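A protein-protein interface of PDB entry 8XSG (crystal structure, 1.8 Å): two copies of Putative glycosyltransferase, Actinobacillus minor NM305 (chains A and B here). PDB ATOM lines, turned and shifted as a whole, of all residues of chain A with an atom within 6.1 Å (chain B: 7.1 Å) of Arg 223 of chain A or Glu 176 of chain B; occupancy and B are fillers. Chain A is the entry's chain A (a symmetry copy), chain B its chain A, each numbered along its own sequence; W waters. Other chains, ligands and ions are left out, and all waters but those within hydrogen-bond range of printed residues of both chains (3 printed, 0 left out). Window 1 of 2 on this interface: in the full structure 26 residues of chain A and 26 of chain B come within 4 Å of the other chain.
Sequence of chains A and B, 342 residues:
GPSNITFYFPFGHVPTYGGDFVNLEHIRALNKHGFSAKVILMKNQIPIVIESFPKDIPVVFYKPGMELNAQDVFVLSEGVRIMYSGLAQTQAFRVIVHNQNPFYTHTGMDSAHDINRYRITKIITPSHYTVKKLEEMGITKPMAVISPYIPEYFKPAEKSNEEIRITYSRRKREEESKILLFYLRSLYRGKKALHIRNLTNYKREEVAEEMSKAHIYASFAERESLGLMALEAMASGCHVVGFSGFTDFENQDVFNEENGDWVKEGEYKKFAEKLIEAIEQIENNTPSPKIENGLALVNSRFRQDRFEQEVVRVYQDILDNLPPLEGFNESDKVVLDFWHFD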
ATOM      1  N   PRO A 102      -9.992  -8.058  18.873  1.00  0.00           N
ATOM      2  CA  PRO A 102     -10.825  -7.244  17.989  1.00  0.00           C
ATOM      3  C   PRO A 102     -12.191  -6.904  18.587  1.00  0.00           C
ATOM      4  O   PRO A 102     -12.750  -5.829  18.337  1.00  0.00           O
ATOM      5  CB  PRO A 102     -10.920  -8.090  16.730  1.00  0.00           C
ATOM      6  CG  PRO A 102     -10.611  -9.511  17.185  1.00  0.00           C
ATOM      7  CD  PRO A 102      -9.576  -9.316  18.260  1.00  0.00           C
ATOM      8  N   PHE A 103     -12.695  -7.774  19.447  1.00  0.00           N
ATOM      9  CA  PHE A 103     -13.961  -7.463  20.114  1.00  0.00           C
ATOM     10  C   PHE A 103     -13.812  -6.428  21.226  1.00  0.00           C
ATOM     11  O   PHE A 103     -14.819  -5.838  21.633  1.00  0.00           O
ATOM     12  CB  PHE A 103     -14.596  -8.750  20.653  1.00  0.00           C
ATOM     13  CG  PHE A 103     -14.882  -9.737  19.563  1.00  0.00           C
ATOM     14  CD1 PHE A 103     -15.944  -9.547  18.681  1.00  0.00           C
ATOM     15  CD2 PHE A 103     -14.057 -10.820  19.374  1.00  0.00           C
ATOM     16  CE1 PHE A 103     -16.200 -10.463  17.677  1.00  0.00           C
ATOM     17  CE2 PHE A 103     -14.304 -11.726  18.347  1.00  0.00           C
ATOM     18  CZ  PHE A 103     -15.392 -11.569  17.525  1.00  0.00           C
ATOM     19  N   LYS A 172     -12.960 -18.266  30.689  1.00  0.00           N
ATOM     20  CA  LYS A 172     -14.117 -17.825  29.919  1.00  0.00           C
ATOM     21  C   LYS A 172     -15.230 -18.844  30.108  1.00  0.00           C
ATOM     22  O   LYS A 172     -14.964 -20.022  30.301  1.00  0.00           O
ATOM     23  CB  LYS A 172     -13.739 -17.712  28.434  1.00  0.00           C
ATOM     24  CG  LYS A 172     -12.593 -16.756  28.183  1.00  0.00           C
ATOM     25  CD  LYS A 172     -12.169 -16.621  26.768  1.00  0.00           C
ATOM     26  CE  LYS A 172     -11.072 -15.608  26.609  1.00  0.00           C
ATOM     27  NZ  LYS A 172     -10.912 -15.239  25.183  1.00  0.00           N
ATOM     28  N   ARG A 173     -16.475 -18.376  29.995  1.00  0.00           N
ATOM     29  CA  ARG A 173     -17.636 -19.255  30.040  1.00  0.00           C
ATOM     30  C   ARG A 173     -17.723 -20.069  31.327  1.00  0.00           C
ATOM     31  O   ARG A 173     -18.164 -21.224  31.309  1.00  0.00           O
ATOM     32  CB  ARG A 173     -17.641 -20.271  28.891  1.00  0.00           C
ATOM     33  CG  ARG A 173     -17.428 -19.718  27.499  1.00  0.00           C
ATOM     34  CD  ARG A 173     -17.740 -20.798  26.486  1.00  0.00           C
ATOM     35  NE  ARG A 173     -17.449 -20.396  25.098  1.00  0.00           N
ATOM     36  CZ  ARG A 173     -18.348 -20.131  24.166  1.00  0.00           C
ATOM     37  NH1 ARG A 173     -19.635 -20.037  24.477  1.00  0.00           N
ATOM     38  NH2 ARG A 173     -17.978 -19.929  22.913  1.00  0.00           N
ATOM     39  N   ALA A 221     -13.189 -21.849  24.963  1.00  0.00           N
ATOM     40  CA  ALA A 221     -12.810 -20.659  24.230  1.00  0.00           C
ATOM     41  C   ALA A 221     -14.007 -19.808  23.823  1.00  0.00           C
ATOM     42  O   ALA A 221     -15.104 -20.322  23.517  1.00  0.00           O
ATOM     43  CB  ALA A 221     -12.046 -21.076  23.017  1.00  0.00           C
ATOM     44  N   GLU A 222     -13.773 -18.496  23.776  1.00  0.00           N
ATOM     45  CA  GLU A 222     -14.863 -17.554  23.480  1.00  0.00           C
ATOM     46  C   GLU A 222     -14.320 -16.282  22.847  1.00  0.00           C
ATOM     47  O   GLU A 222     -13.469 -15.619  23.453  1.00  0.00           O
ATOM     48  CB  GLU A 222     -15.587 -17.245  24.774  1.00  0.00           C
ATOM     49  CG  GLU A 222     -16.844 -16.405  24.637  1.00  0.00           C
ATOM     50  CD  GLU A 222     -17.470 -16.128  26.011  1.00  0.00           C
ATOM     51  OE1 GLU A 222     -16.715 -15.674  26.952  1.00  0.00           O
ATOM     52  OE2 GLU A 222     -18.731 -16.305  26.146  1.00  0.00           O
ATOM     53  N   ARG A 223     -14.887 -15.925  21.692  1.00  0.00           N
ATOM     54  CA  ARG A 223     -14.549 -14.699  20.963  1.00  0.00           C
ATOM     55  C   ARG A 223     -13.032 -14.524  20.892  1.00  0.00           C
ATOM     56  O   ARG A 223     -12.489 -13.455  21.232  1.00  0.00           O
ATOM     57  CB  ARG A 223     -15.273 -13.474  21.539  1.00  0.00           C
ATOM     58  CG  ARG A 223     -16.709 -13.373  21.049  1.00  0.00           C
ATOM     59  CD  ARG A 223     -17.384 -12.084  21.421  1.00  0.00           C
ATOM     60  NE  ARG A 223     -17.569 -11.999  22.867  1.00  0.00           N
ATOM     61  CZ  ARG A 223     -18.449 -12.693  23.579  1.00  0.00           C
ATOM     62  NH1 ARG A 223     -19.372 -13.447  22.990  1.00  0.00           N
ATOM     63  NH2 ARG A 223     -18.399 -12.618  24.901  1.00  0.00           N
ATOM     64  N   GLU A 224     -12.375 -15.596  20.422  1.00  0.00           N
ATOM     65  CA  GLU A 224     -10.930 -15.606  20.224  1.00  0.00           C
ATOM     66  C   GLU A 224     -10.511 -14.922  18.908  1.00  0.00           C
ATOM     67  O   GLU A 224     -11.281 -14.764  17.943  1.00  0.00           O
ATOM     68  CB  GLU A 224     -10.436 -17.054  20.177  1.00  0.00           C
ATOM     69  CG  GLU A 224     -10.809 -17.895  21.383  1.00  0.00           C
ATOM     70  CD  GLU A 224     -10.249 -17.443  22.713  1.00  0.00           C
ATOM     71  OE1 GLU A 224      -9.203 -16.767  22.684  1.00  0.00           O
ATOM     72  OE2 GLU A 224     -10.894 -17.718  23.781  1.00  0.00           O
ATOM     73  N   SER A 225      -9.239 -14.503  18.878  1.00  0.00           N
ATOM     74  CA  SER A 225      -8.561 -14.102  17.655  1.00  0.00           C
ATOM     75  C   SER A 225      -7.806 -15.289  17.042  1.00  0.00           C
ATOM     76  O   SER A 225      -7.740 -15.437  15.814  1.00  0.00           O
ATOM     77  CB  SER A 225      -7.610 -12.966  17.929  1.00  0.00           C
ATOM     78  OG  SER A 225      -6.745 -13.268  19.017  1.00  0.00           O
ATOM     79  N   GLY A 245     -14.070 -21.134  19.962  1.00  0.00           N
ATOM     80  CA  GLY A 245     -13.796 -19.729  20.123  1.00  0.00           C
ATOM     81  C   GLY A 245     -14.188 -18.855  18.933  1.00  0.00           C
ATOM     82  O   GLY A 245     -13.974 -17.642  19.019  1.00  0.00           O
ATOM     83  N   PHE A 246     -14.771 -19.451  17.880  1.00  0.00           N
ATOM     84  CA  PHE A 246     -15.126 -18.756  16.656  1.00  0.00           C
ATOM     85  C   PHE A 246     -16.552 -19.127  16.234  1.00  0.00           C
ATOM     86  O   PHE A 246     -16.786 -20.220  15.734  1.00  0.00           O
ATOM     87  CB  PHE A 246     -14.172 -19.128  15.516  1.00  0.00           C
ATOM     88  CG  PHE A 246     -12.744 -18.823  15.870  1.00  0.00           C
ATOM     89  CD1 PHE A 246     -11.968 -19.736  16.565  1.00  0.00           C
ATOM     90  CD2 PHE A 246     -12.206 -17.596  15.540  1.00  0.00           C
ATOM     91  CE1 PHE A 246     -10.671 -19.420  16.927  1.00  0.00           C
ATOM     92  CE2 PHE A 246     -10.914 -17.279  15.901  1.00  0.00           C
ATOM     93  CZ  PHE A 246     -10.143 -18.199  16.564  1.00  0.00           C
ATOM     94  N   THR A 247     -17.511 -18.237  16.504  1.00  0.00           N
ATOM     95  CA  THR A 247     -18.873 -18.450  16.024  1.00  0.00           C
ATOM     96  C   THR A 247     -18.933 -18.550  14.504  1.00  0.00           C
ATOM     97  O   THR A 247     -19.655 -19.390  13.918  1.00  0.00           O
ATOM     98  CB  THR A 247     -19.802 -17.353  16.559  1.00  0.00           C
ATOM     99  OG1 THR A 247     -19.351 -16.073  16.121  1.00  0.00           O
ATOM    100  CG2 THR A 247     -19.921 -17.385  18.068  1.00  0.00           C
ATOM    101  N   LYS B 172     -28.165  -9.521  30.639  1.00  0.00           N
ATOM    102  CA  LYS B 172     -27.375 -10.609  30.074  1.00  0.00           C
ATOM    103  C   LYS B 172     -26.518 -10.041  28.953  1.00  0.00           C
ATOM    104  O   LYS B 172     -26.912  -9.087  28.296  1.00  0.00           O
ATOM    105  CB  LYS B 172     -28.310 -11.701  29.534  1.00  0.00           C
ATOM    106  CG  LYS B 172     -29.235 -12.268  30.591  1.00  0.00           C
ATOM    107  CD  LYS B 172     -30.176 -13.314  30.123  1.00  0.00           C
ATOM    108  CE  LYS B 172     -31.008 -13.859  31.249  1.00  0.00           C
ATOM    109  NZ  LYS B 172     -31.673 -15.117  30.839  1.00  0.00           N
ATOM    110  N   ARG B 173     -25.370 -10.678  28.716  1.00  0.00           N
ATOM    111  CA  ARG B 173     -24.503 -10.317  27.602  1.00  0.00           C
ATOM    112  C   ARG B 173     -24.051  -8.860  27.642  1.00  0.00           C
ATOM    113  O   ARG B 173     -23.904  -8.222  26.593  1.00  0.00           O
ATOM    114  CB  ARG B 173     -25.188 -10.514  26.244  1.00  0.00           C
ATOM    115  CG  ARG B 173     -25.848 -11.855  26.010  1.00  0.00           C
ATOM    116  CD  ARG B 173     -26.218 -11.974  24.547  1.00  0.00           C
ATOM    117  NE  ARG B 173     -26.977 -13.198  24.236  1.00  0.00           N
ATOM    118  CZ  ARG B 173     -26.519 -14.241  23.563  1.00  0.00           C
ATOM    119  NH1 ARG B 173     -25.232 -14.333  23.256  1.00  0.00           N
ATOM    120  NH2 ARG B 173     -27.332 -15.221  23.208  1.00  0.00           N
ATOM    121  N   GLU B 174     -23.737  -8.327  28.814  1.00  0.00           N
ATOM    122  CA  GLU B 174     -23.341  -6.929  28.889  1.00  0.00           C
ATOM    123  C   GLU B 174     -22.173  -6.631  27.929  1.00  0.00           C
ATOM    124  O   GLU B 174     -22.187  -5.636  27.231  1.00  0.00           O
ATOM    125  CB  GLU B 174     -22.988  -6.553  30.322  1.00  0.00           C
ATOM    126  CG  GLU B 174     -22.474  -5.121  30.412  1.00  0.00           C
ATOM    127  CD  GLU B 174     -22.384  -4.567  31.811  1.00  0.00           C
ATOM    128  OE1 GLU B 174     -22.405  -5.358  32.748  1.00  0.00           O
ATOM    129  OE2 GLU B 174     -22.269  -3.354  31.938  1.00  0.00           O
ATOM    130  N   GLU B 175     -21.133  -7.462  27.919  1.00  0.00           N
ATOM    131  CA  GLU B 175     -19.976  -7.184  27.075  1.00  0.00           C
ATOM    132  C   GLU B 175     -20.384  -7.209  25.608  1.00  0.00           C
ATOM    133  O   GLU B 175     -19.945  -6.382  24.806  1.00  0.00           O
ATOM    134  CB  GLU B 175     -18.836  -8.161  27.397  1.00  0.00           C
ATOM    135  CG  GLU B 175     -17.650  -7.932  26.513  1.00  0.00           C
ATOM    136  CD  GLU B 175     -17.060  -6.529  26.594  1.00  0.00           C
ATOM    137  OE1 GLU B 175     -17.147  -5.871  27.695  1.00  0.00           O
ATOM    138  OE2 GLU B 175     -16.514  -6.088  25.560  1.00  0.00           O
ATOM    139  N   GLU B 176     -21.276  -8.146  25.241  1.00  0.00           N
ATOM    140  CA  GLU B 176     -21.684  -8.223  23.854  1.00  0.00           C
ATOM    141  C   GLU B 176     -22.508  -7.004  23.438  1.00  0.00           C
ATOM    142  O   GLU B 176     -22.491  -6.639  22.264  1.00  0.00           O
ATOM    143  CB  GLU B 176     -22.492  -9.479  23.596  1.00  0.00           C
ATOM    144  CG  GLU B 176     -21.697 -10.770  23.799  1.00  0.00           C
ATOM    145  CD  GLU B 176     -22.494 -11.942  23.265  1.00  0.00           C
ATOM    146  OE1 GLU B 176     -22.654 -11.991  22.022  1.00  0.00           O
ATOM    147  OE2 GLU B 176     -22.970 -12.796  24.082  1.00  0.00           O
ATOM    148  N   SER B 177     -23.274  -6.399  24.358  1.00  0.00           N
ATOM    149  CA  SER B 177     -23.988  -5.184  23.997  1.00  0.00           C
ATOM    150  C   SER B 177     -23.008  -4.071  23.615  1.00  0.00           C
ATOM    151  O   SER B 177     -23.294  -3.285  22.737  1.00  0.00           O
ATOM    152  CB  SER B 177     -24.901  -4.753  25.107  1.00  0.00           C
ATOM    153  OG  SER B 177     -24.198  -4.225  26.210  1.00  0.00           O
ATOM    154  N   LYS B 178     -21.821  -4.047  24.230  1.00  0.00           N
ATOM    155  CA  LYS B 178     -20.824  -3.059  23.877  1.00  0.00           C
ATOM    156  C   LYS B 178     -20.238  -3.358  22.492  1.00  0.00           C
ATOM    157  O   LYS B 178     -19.981  -2.439  21.702  1.00  0.00           O
ATOM    158  CB  LYS B 178     -19.740  -3.026  24.968  1.00  0.00           C
ATOM    159  CG  LYS B 178     -20.259  -2.667  26.355  1.00  0.00           C
ATOM    160  CD  LYS B 178     -19.206  -2.651  27.426  1.00  0.00           C
ATOM    161  CE  LYS B 178     -19.797  -2.376  28.790  1.00  0.00           C
ATOM    162  NZ  LYS B 178     -18.815  -2.736  29.826  1.00  0.00           N
ATOM    163  N   ILE B 179     -20.027  -4.635  22.177  1.00  0.00           N
ATOM    164  CA  ILE B 179     -19.571  -5.008  20.849  1.00  0.00           C
ATOM    165  C   ILE B 179     -20.575  -4.598  19.786  1.00  0.00           C
ATOM    166  O   ILE B 179     -20.236  -3.939  18.789  1.00  0.00           O
ATOM    167  CB  ILE B 179     -19.289  -6.517  20.785  1.00  0.00           C
ATOM    168  CG1 ILE B 179     -18.203  -6.946  21.780  1.00  0.00           C
ATOM    169  CG2 ILE B 179     -18.972  -6.898  19.349  1.00  0.00           C
ATOM    170  CD1 ILE B 179     -18.111  -8.464  21.975  1.00  0.00           C
ATOM    171  N   LEU B 180     -21.839  -4.945  20.030  1.00  0.00           N
ATOM    172  CA  LEU B 180     -22.926  -4.575  19.136  1.00  0.00           C
ATOM    173  C   LEU B 180     -22.971  -3.064  18.942  1.00  0.00           C
ATOM    174  O   LEU B 180     -23.085  -2.613  17.807  1.00  0.00           O
ATOM    175  CB  LEU B 180     -24.246  -5.156  19.678  1.00  0.00           C
ATOM    176  CG  LEU B 180     -25.523  -4.894  18.858  1.00  0.00           C
ATOM    177  CD1 LEU B 180     -26.070  -3.489  19.087  1.00  0.00           C
ATOM    178  CD2 LEU B 180     -25.358  -5.138  17.369  1.00  0.00           C
ATOM    179  N   LEU B 181     -22.914  -2.274  20.018  1.00  0.00           N
ATOM    180  CA  LEU B 181     -23.091  -0.842  19.865  1.00  0.00           C
ATOM    181  C   LEU B 181     -21.928  -0.271  19.061  1.00  0.00           C
ATOM    182  O   LEU B 181     -22.114   0.690  18.318  1.00  0.00           O
ATOM    183  CB  LEU B 181     -23.291  -0.154  21.228  1.00  0.00           C
ATOM    184  CG  LEU B 181     -24.644  -0.455  21.890  1.00  0.00           C
ATOM    185  CD1 LEU B 181     -24.706   0.080  23.299  1.00  0.00           C
ATOM    186  CD2 LEU B 181     -25.827   0.088  21.105  1.00  0.00           C
ATOM    187  N   PHE B 182     -20.744  -0.894  19.177  1.00  0.00           N
ATOM    188  CA  PHE B 182     -19.609  -0.470  18.376  1.00  0.00           C
ATOM    189  C   PHE B 182     -19.898  -0.686  16.896  1.00  0.00           C
ATOM    190  O   PHE B 182     -19.613   0.177  16.077  1.00  0.00           O
ATOM    191  CB  PHE B 182     -18.328  -1.199  18.823  1.00  0.00           C
ATOM    192  CG  PHE B 182     -17.100  -0.852  18.021  1.00  0.00           C
ATOM    193  CD1 PHE B 182     -16.788  -1.545  16.873  1.00  0.00           C
ATOM    194  CD2 PHE B 182     -16.242   0.161  18.427  1.00  0.00           C
ATOM    195  CE1 PHE B 182     -15.684  -1.204  16.115  1.00  0.00           C
ATOM    196  CE2 PHE B 182     -15.127   0.490  17.674  1.00  0.00           C
ATOM    197  CZ  PHE B 182     -14.866  -0.175  16.508  1.00  0.00           C
ATOM    198  N   PHE B 220     -30.828  -8.911  23.945  1.00  0.00           N
ATOM    199  CA  PHE B 220     -29.632  -9.620  24.375  1.00  0.00           C
ATOM    200  C   PHE B 220     -29.966 -10.861  25.208  1.00  0.00           C
ATOM    201  O   PHE B 220     -29.184 -11.307  26.047  1.00  0.00           O
ATOM    202  CB  PHE B 220     -28.711  -8.645  25.097  1.00  0.00           C
ATOM    203  CG  PHE B 220     -28.118  -7.655  24.150  1.00  0.00           C
ATOM    204  CD1 PHE B 220     -27.017  -8.005  23.372  1.00  0.00           C
ATOM    205  CD2 PHE B 220     -28.717  -6.424  23.945  1.00  0.00           C
ATOM    206  CE1 PHE B 220     -26.524  -7.105  22.442  1.00  0.00           C
ATOM    207  CE2 PHE B 220     -28.188  -5.518  23.036  1.00  0.00           C
ATOM    208  CZ  PHE B 220     -27.099  -5.875  22.268  1.00  0.00           C
ATOM    209  N   ALA B 221     -31.096 -11.499  24.881  1.00  0.00           N
ATOM    210  CA  ALA B 221     -31.498 -12.727  25.533  1.00  0.00           C
ATOM    211  C   ALA B 221     -30.437 -13.818  25.445  1.00  0.00           C
ATOM    212  O   ALA B 221     -29.701 -13.937  24.443  1.00  0.00           O
ATOM    213  CB  ALA B 221     -32.768 -13.201  24.908  1.00  0.00           C
ATOM    214  N   GLU B 222     -30.397 -14.647  26.488  1.00  0.00           N
ATOM    215  CA  GLU B 222     -29.366 -15.693  26.571  1.00  0.00           C
ATOM    216  C   GLU B 222     -29.853 -16.868  27.405  1.00  0.00           C
ATOM    217  O   GLU B 222     -30.216 -16.672  28.573  1.00  0.00           O
ATOM    218  CB  GLU B 222     -28.119 -15.082  27.176  1.00  0.00           C
ATOM    219  CG  GLU B 222     -26.893 -15.979  27.197  1.00  0.00           C
ATOM    220  CD  GLU B 222     -25.707 -15.268  27.862  1.00  0.00           C
ATOM    221  OE1 GLU B 222     -25.887 -14.711  29.010  1.00  0.00           O
ATOM    222  OE2 GLU B 222     -24.571 -15.312  27.272  1.00  0.00           O
ATOM    223  N   PHE B 243     -30.707 -11.220  19.533  1.00  0.00           N
ATOM    224  CA  PHE B 243     -30.550 -12.600  19.946  1.00  0.00           C
ATOM    225  C   PHE B 243     -31.889 -13.115  20.446  1.00  0.00           C
ATOM    226  O   PHE B 243     -32.614 -12.381  21.125  1.00  0.00           O
ATOM    227  CB  PHE B 243     -29.473 -12.713  21.021  1.00  0.00           C
ATOM    228  CG  PHE B 243     -28.088 -12.316  20.568  1.00  0.00           C
ATOM    229  CD1 PHE B 243     -27.461 -12.999  19.536  1.00  0.00           C
ATOM    230  CD2 PHE B 243     -27.392 -11.294  21.190  1.00  0.00           C
ATOM    231  CE1 PHE B 243     -26.192 -12.624  19.117  1.00  0.00           C
ATOM    232  CE2 PHE B 243     -26.120 -10.924  20.769  1.00  0.00           C
ATOM    233  CZ  PHE B 243     -25.504 -11.624  19.768  1.00  0.00           C
ATOM    234  N   LYS B 264     -28.113 -15.029  14.883  1.00  0.00           N
ATOM    235  CA  LYS B 264     -27.449 -16.125  15.571  1.00  0.00           C
ATOM    236  C   LYS B 264     -26.258 -15.588  16.354  1.00  0.00           C
ATOM    237  O   LYS B 264     -25.892 -14.425  16.232  1.00  0.00           O
ATOM    238  CB  LYS B 264     -27.055 -17.233  14.595  1.00  0.00           C
ATOM    239  CG  LYS B 264     -28.244 -17.960  13.934  1.00  0.00           C
ATOM    240  CD  LYS B 264     -27.868 -19.011  12.866  1.00  0.00           C
ATOM    241  CE  LYS B 264     -26.868 -20.085  13.283  1.00  0.00           C
ATOM    242  NZ  LYS B 264     -27.480 -21.293  13.907  1.00  0.00           N
ATOM    243  N   GLU B 265     -25.684 -16.447  17.190  1.00  0.00           N
ATOM    244  CA  GLU B 265     -24.545 -16.075  18.016  1.00  0.00           C
ATOM    245  C   GLU B 265     -23.486 -15.443  17.128  1.00  0.00           C
ATOM    246  O   GLU B 265     -23.186 -15.914  16.038  1.00  0.00           O
ATOM    247  CB  GLU B 265     -23.972 -17.317  18.708  1.00  0.00           C
ATOM    248  CG  GLU B 265     -24.916 -17.915  19.749  1.00  0.00           C
ATOM    249  CD  GLU B 265     -25.113 -17.125  21.022  1.00  0.00           C
ATOM    250  OE1 GLU B 265     -24.194 -16.383  21.425  1.00  0.00           O
ATOM    251  OE2 GLU B 265     -26.188 -17.317  21.655  1.00  0.00           O
ATOM    252  N   GLY B 266     -22.878 -14.400  17.675  1.00  0.00           N
ATOM    253  CA  GLY B 266     -21.762 -13.698  17.085  1.00  0.00           C
ATOM    254  C   GLY B 266     -22.110 -12.864  15.853  1.00  0.00           C
ATOM    255  O   GLY B 266     -21.227 -12.228  15.310  1.00  0.00           O
ATOM    256  N   GLU B 267     -23.386 -12.760  15.454  1.00  0.00           N
ATOM    257  CA  GLU B 267     -23.736 -12.069  14.214  1.00  0.00           C
ATOM    258  C   GLU B 267     -23.965 -10.579  14.496  1.00  0.00           C
ATOM    259  O   GLU B 267     -25.048 -10.037  14.286  1.00  0.00           O
ATOM    260  CB  GLU B 267     -24.954 -12.752  13.573  1.00  0.00           C
ATOM    261  CG  GLU B 267     -24.665 -14.162  13.061  1.00  0.00           C
ATOM    262  CD  GLU B 267     -25.766 -14.718  12.156  1.00  0.00           C
ATOM    263  OE1 GLU B 267     -26.945 -14.416  12.385  1.00  0.00           O
ATOM    264  OE2 GLU B 267     -25.456 -15.451  11.203  1.00  0.00           O
ATOM    265  N   TYR B 268     -22.914  -9.880  14.944  1.00  0.00           N
ATOM    266  CA  TYR B 268     -23.032  -8.491  15.356  1.00  0.00           C
ATOM    267  C   TYR B 268     -23.320  -7.597  14.152  1.00  0.00           C
ATOM    268  O   TYR B 268     -24.079  -6.630  14.268  1.00  0.00           O
ATOM    269  CB  TYR B 268     -21.786  -8.006  16.112  1.00  0.00           C
ATOM    270  CG  TYR B 268     -21.453  -8.877  17.287  1.00  0.00           C
ATOM    271  CD1 TYR B 268     -22.275  -8.900  18.387  1.00  0.00           C
ATOM    272  CD2 TYR B 268     -20.333  -9.694  17.314  1.00  0.00           C
ATOM    273  CE1 TYR B 268     -22.015  -9.707  19.470  1.00  0.00           C
ATOM    274  CE2 TYR B 268     -20.064 -10.518  18.385  1.00  0.00           C
ATOM    275  CZ  TYR B 268     -20.905 -10.521  19.485  1.00  0.00           C
ATOM    276  OH  TYR B 268     -20.691 -11.359  20.554  1.00  0.00           O
ATOM    277  N   PHE B 271     -26.906  -8.054  13.220  1.00  0.00           N
ATOM    278  CA  PHE B 271     -27.677  -7.404  14.275  1.00  0.00           C
ATOM    279  C   PHE B 271     -27.710  -5.897  14.011  1.00  0.00           C
ATOM    280  O   PHE B 271     -28.785  -5.274  13.987  1.00  0.00           O
ATOM    281  CB  PHE B 271     -27.096  -7.802  15.635  1.00  0.00           C
ATOM    282  CG  PHE B 271     -27.866  -7.544  16.908  1.00  0.00           C
ATOM    283  CD1 PHE B 271     -28.904  -6.624  16.998  1.00  0.00           C
ATOM    284  CD2 PHE B 271     -27.489  -8.236  18.058  1.00  0.00           C
ATOM    285  CE1 PHE B 271     -29.513  -6.364  18.215  1.00  0.00           C
ATOM    286  CE2 PHE B 271     -28.111  -7.997  19.273  1.00  0.00           C
ATOM    287  CZ  PHE B 271     -29.161  -7.082  19.337  1.00  0.00           C
HETATM  288  O   HOH W   1     -20.021 -14.452  20.224  1.00  0.00           O
HETATM  289  O   HOH W   2     -21.138 -15.484  14.083  1.00  0.00           O
HETATM  290  O   HOH W   3     -15.357  -7.728  23.791  1.00  0.00           O
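The side-chain carboxylate of Glu 176 of chain B is in salt-bridge range of the guanidinium group of Arg 223 of chain A, at 3.7 Å.
The guanidinium group (NH1) of Arg 223 of chain A is in hydrogen-bond range of the side-chain hydroxyl (OH) of Tyr 268 of chain B (3.5 Å).
Water W3 lies within hydrogen-bond range of OE2 of Glu 175 of chain B and O of Phe 103 of chain A.
Water W2 lies within hydrogen-bond range of OG1 of Thr 247 of chain A (2.8 Å), O of Glu 265 of chain B (2.9 Å) and O of Gly 266 of chain B (3.5 Å).
Water W1 lies within hydrogen-bond range of the guanidinium group of Arg 223 of chain A (3.0 Å) and the side-chain hydroxyl of Tyr 268 of chain B (3.2 Å).
Of the 21 printed residues of chain B, 5 touch a printed residue of chain A.
Along chain B the printed residues that touch a printed residue of chain A span positions 176 to 268.
Printed residues of chain A that touch a printed residue of chain B: Phe 103, Arg 223 and Thr 247.
Among the printed residues, 7 pairs touch across the chains.
CG1 of Ile 179 of chain B touches O of Phe 103 of chain A (3.6 Å).
Phe 103 of chain A touches Tyr 268 of chain B (CE1 to CE2, 3.9 Å).
Arg 223 of chain A touches Ile 179 of chain B (NE to CD1, 3.7 Å).
CB of Thr 247 of chain A touches O of Glu 265 of chain B, 3.7 Å away.
Thr 247 of chain A touches Gly 266 of chain B.
Positions printed for both chains: 172, 173, 221 and 222.
Of the 7 pairs that touch across the chains among the printed residues, none has its exchanged pair printed and touching as well.
Of the printed residues of chain B, Phe 103 of chain A touches Ile 179 and Tyr 268.
Glu 176 of chain B touches one residue of chain A.
Lys 178 of chain B touches none of the printed residues of chain A.
Of the printed residues of chain A, Ile 179 of chain B touches Phe 103 and Arg 223.
Of the printed residues of chain A, Glu 265 of chain B touches Thr 247.
Of the printed residues of chain A, Gly 266 of chain B touches Thr 247 (3.5 Å).
Of the printed residues of chain A, Tyr 268 of chain B touches Phe 103 and Arg 223.
The nearest residue of chain A that does not touch Glu 176 of chain B is Glu 222 of chain A (5.9 Å).
The nearest printed residue of chain A that does not touch Tyr 268 of chain B is Thr 247 of chain A (6.0 Å).
The backbone carbonyl oxygen of Gly 245 of chain A is in hydrogen-bond range of the backbone NH of Arg 223 of chain A (3.3 Å).
The guanidinium group (NH1) of Arg 173 of chain B is in salt-bridge range of the side-chain carboxylate (OE2) of Glu 176 of chain B, 2.9 Å away.
The side-chain carboxylate (OE2) of Glu 222 of chain A is in salt-bridge range of the guanidinium group (NH2) of Arg 223 of chain A.
OE1 of Glu 176 of chain B lies within hydrogen-bond range of OH of Tyr 268 of chain B, at 2.5 Å.
The guanidinium group (NH2) of Arg 173 of chain B lies within salt-bridge range of the side-chain carboxylate (OE2) of Glu 265 of chain B (2.8 Å).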
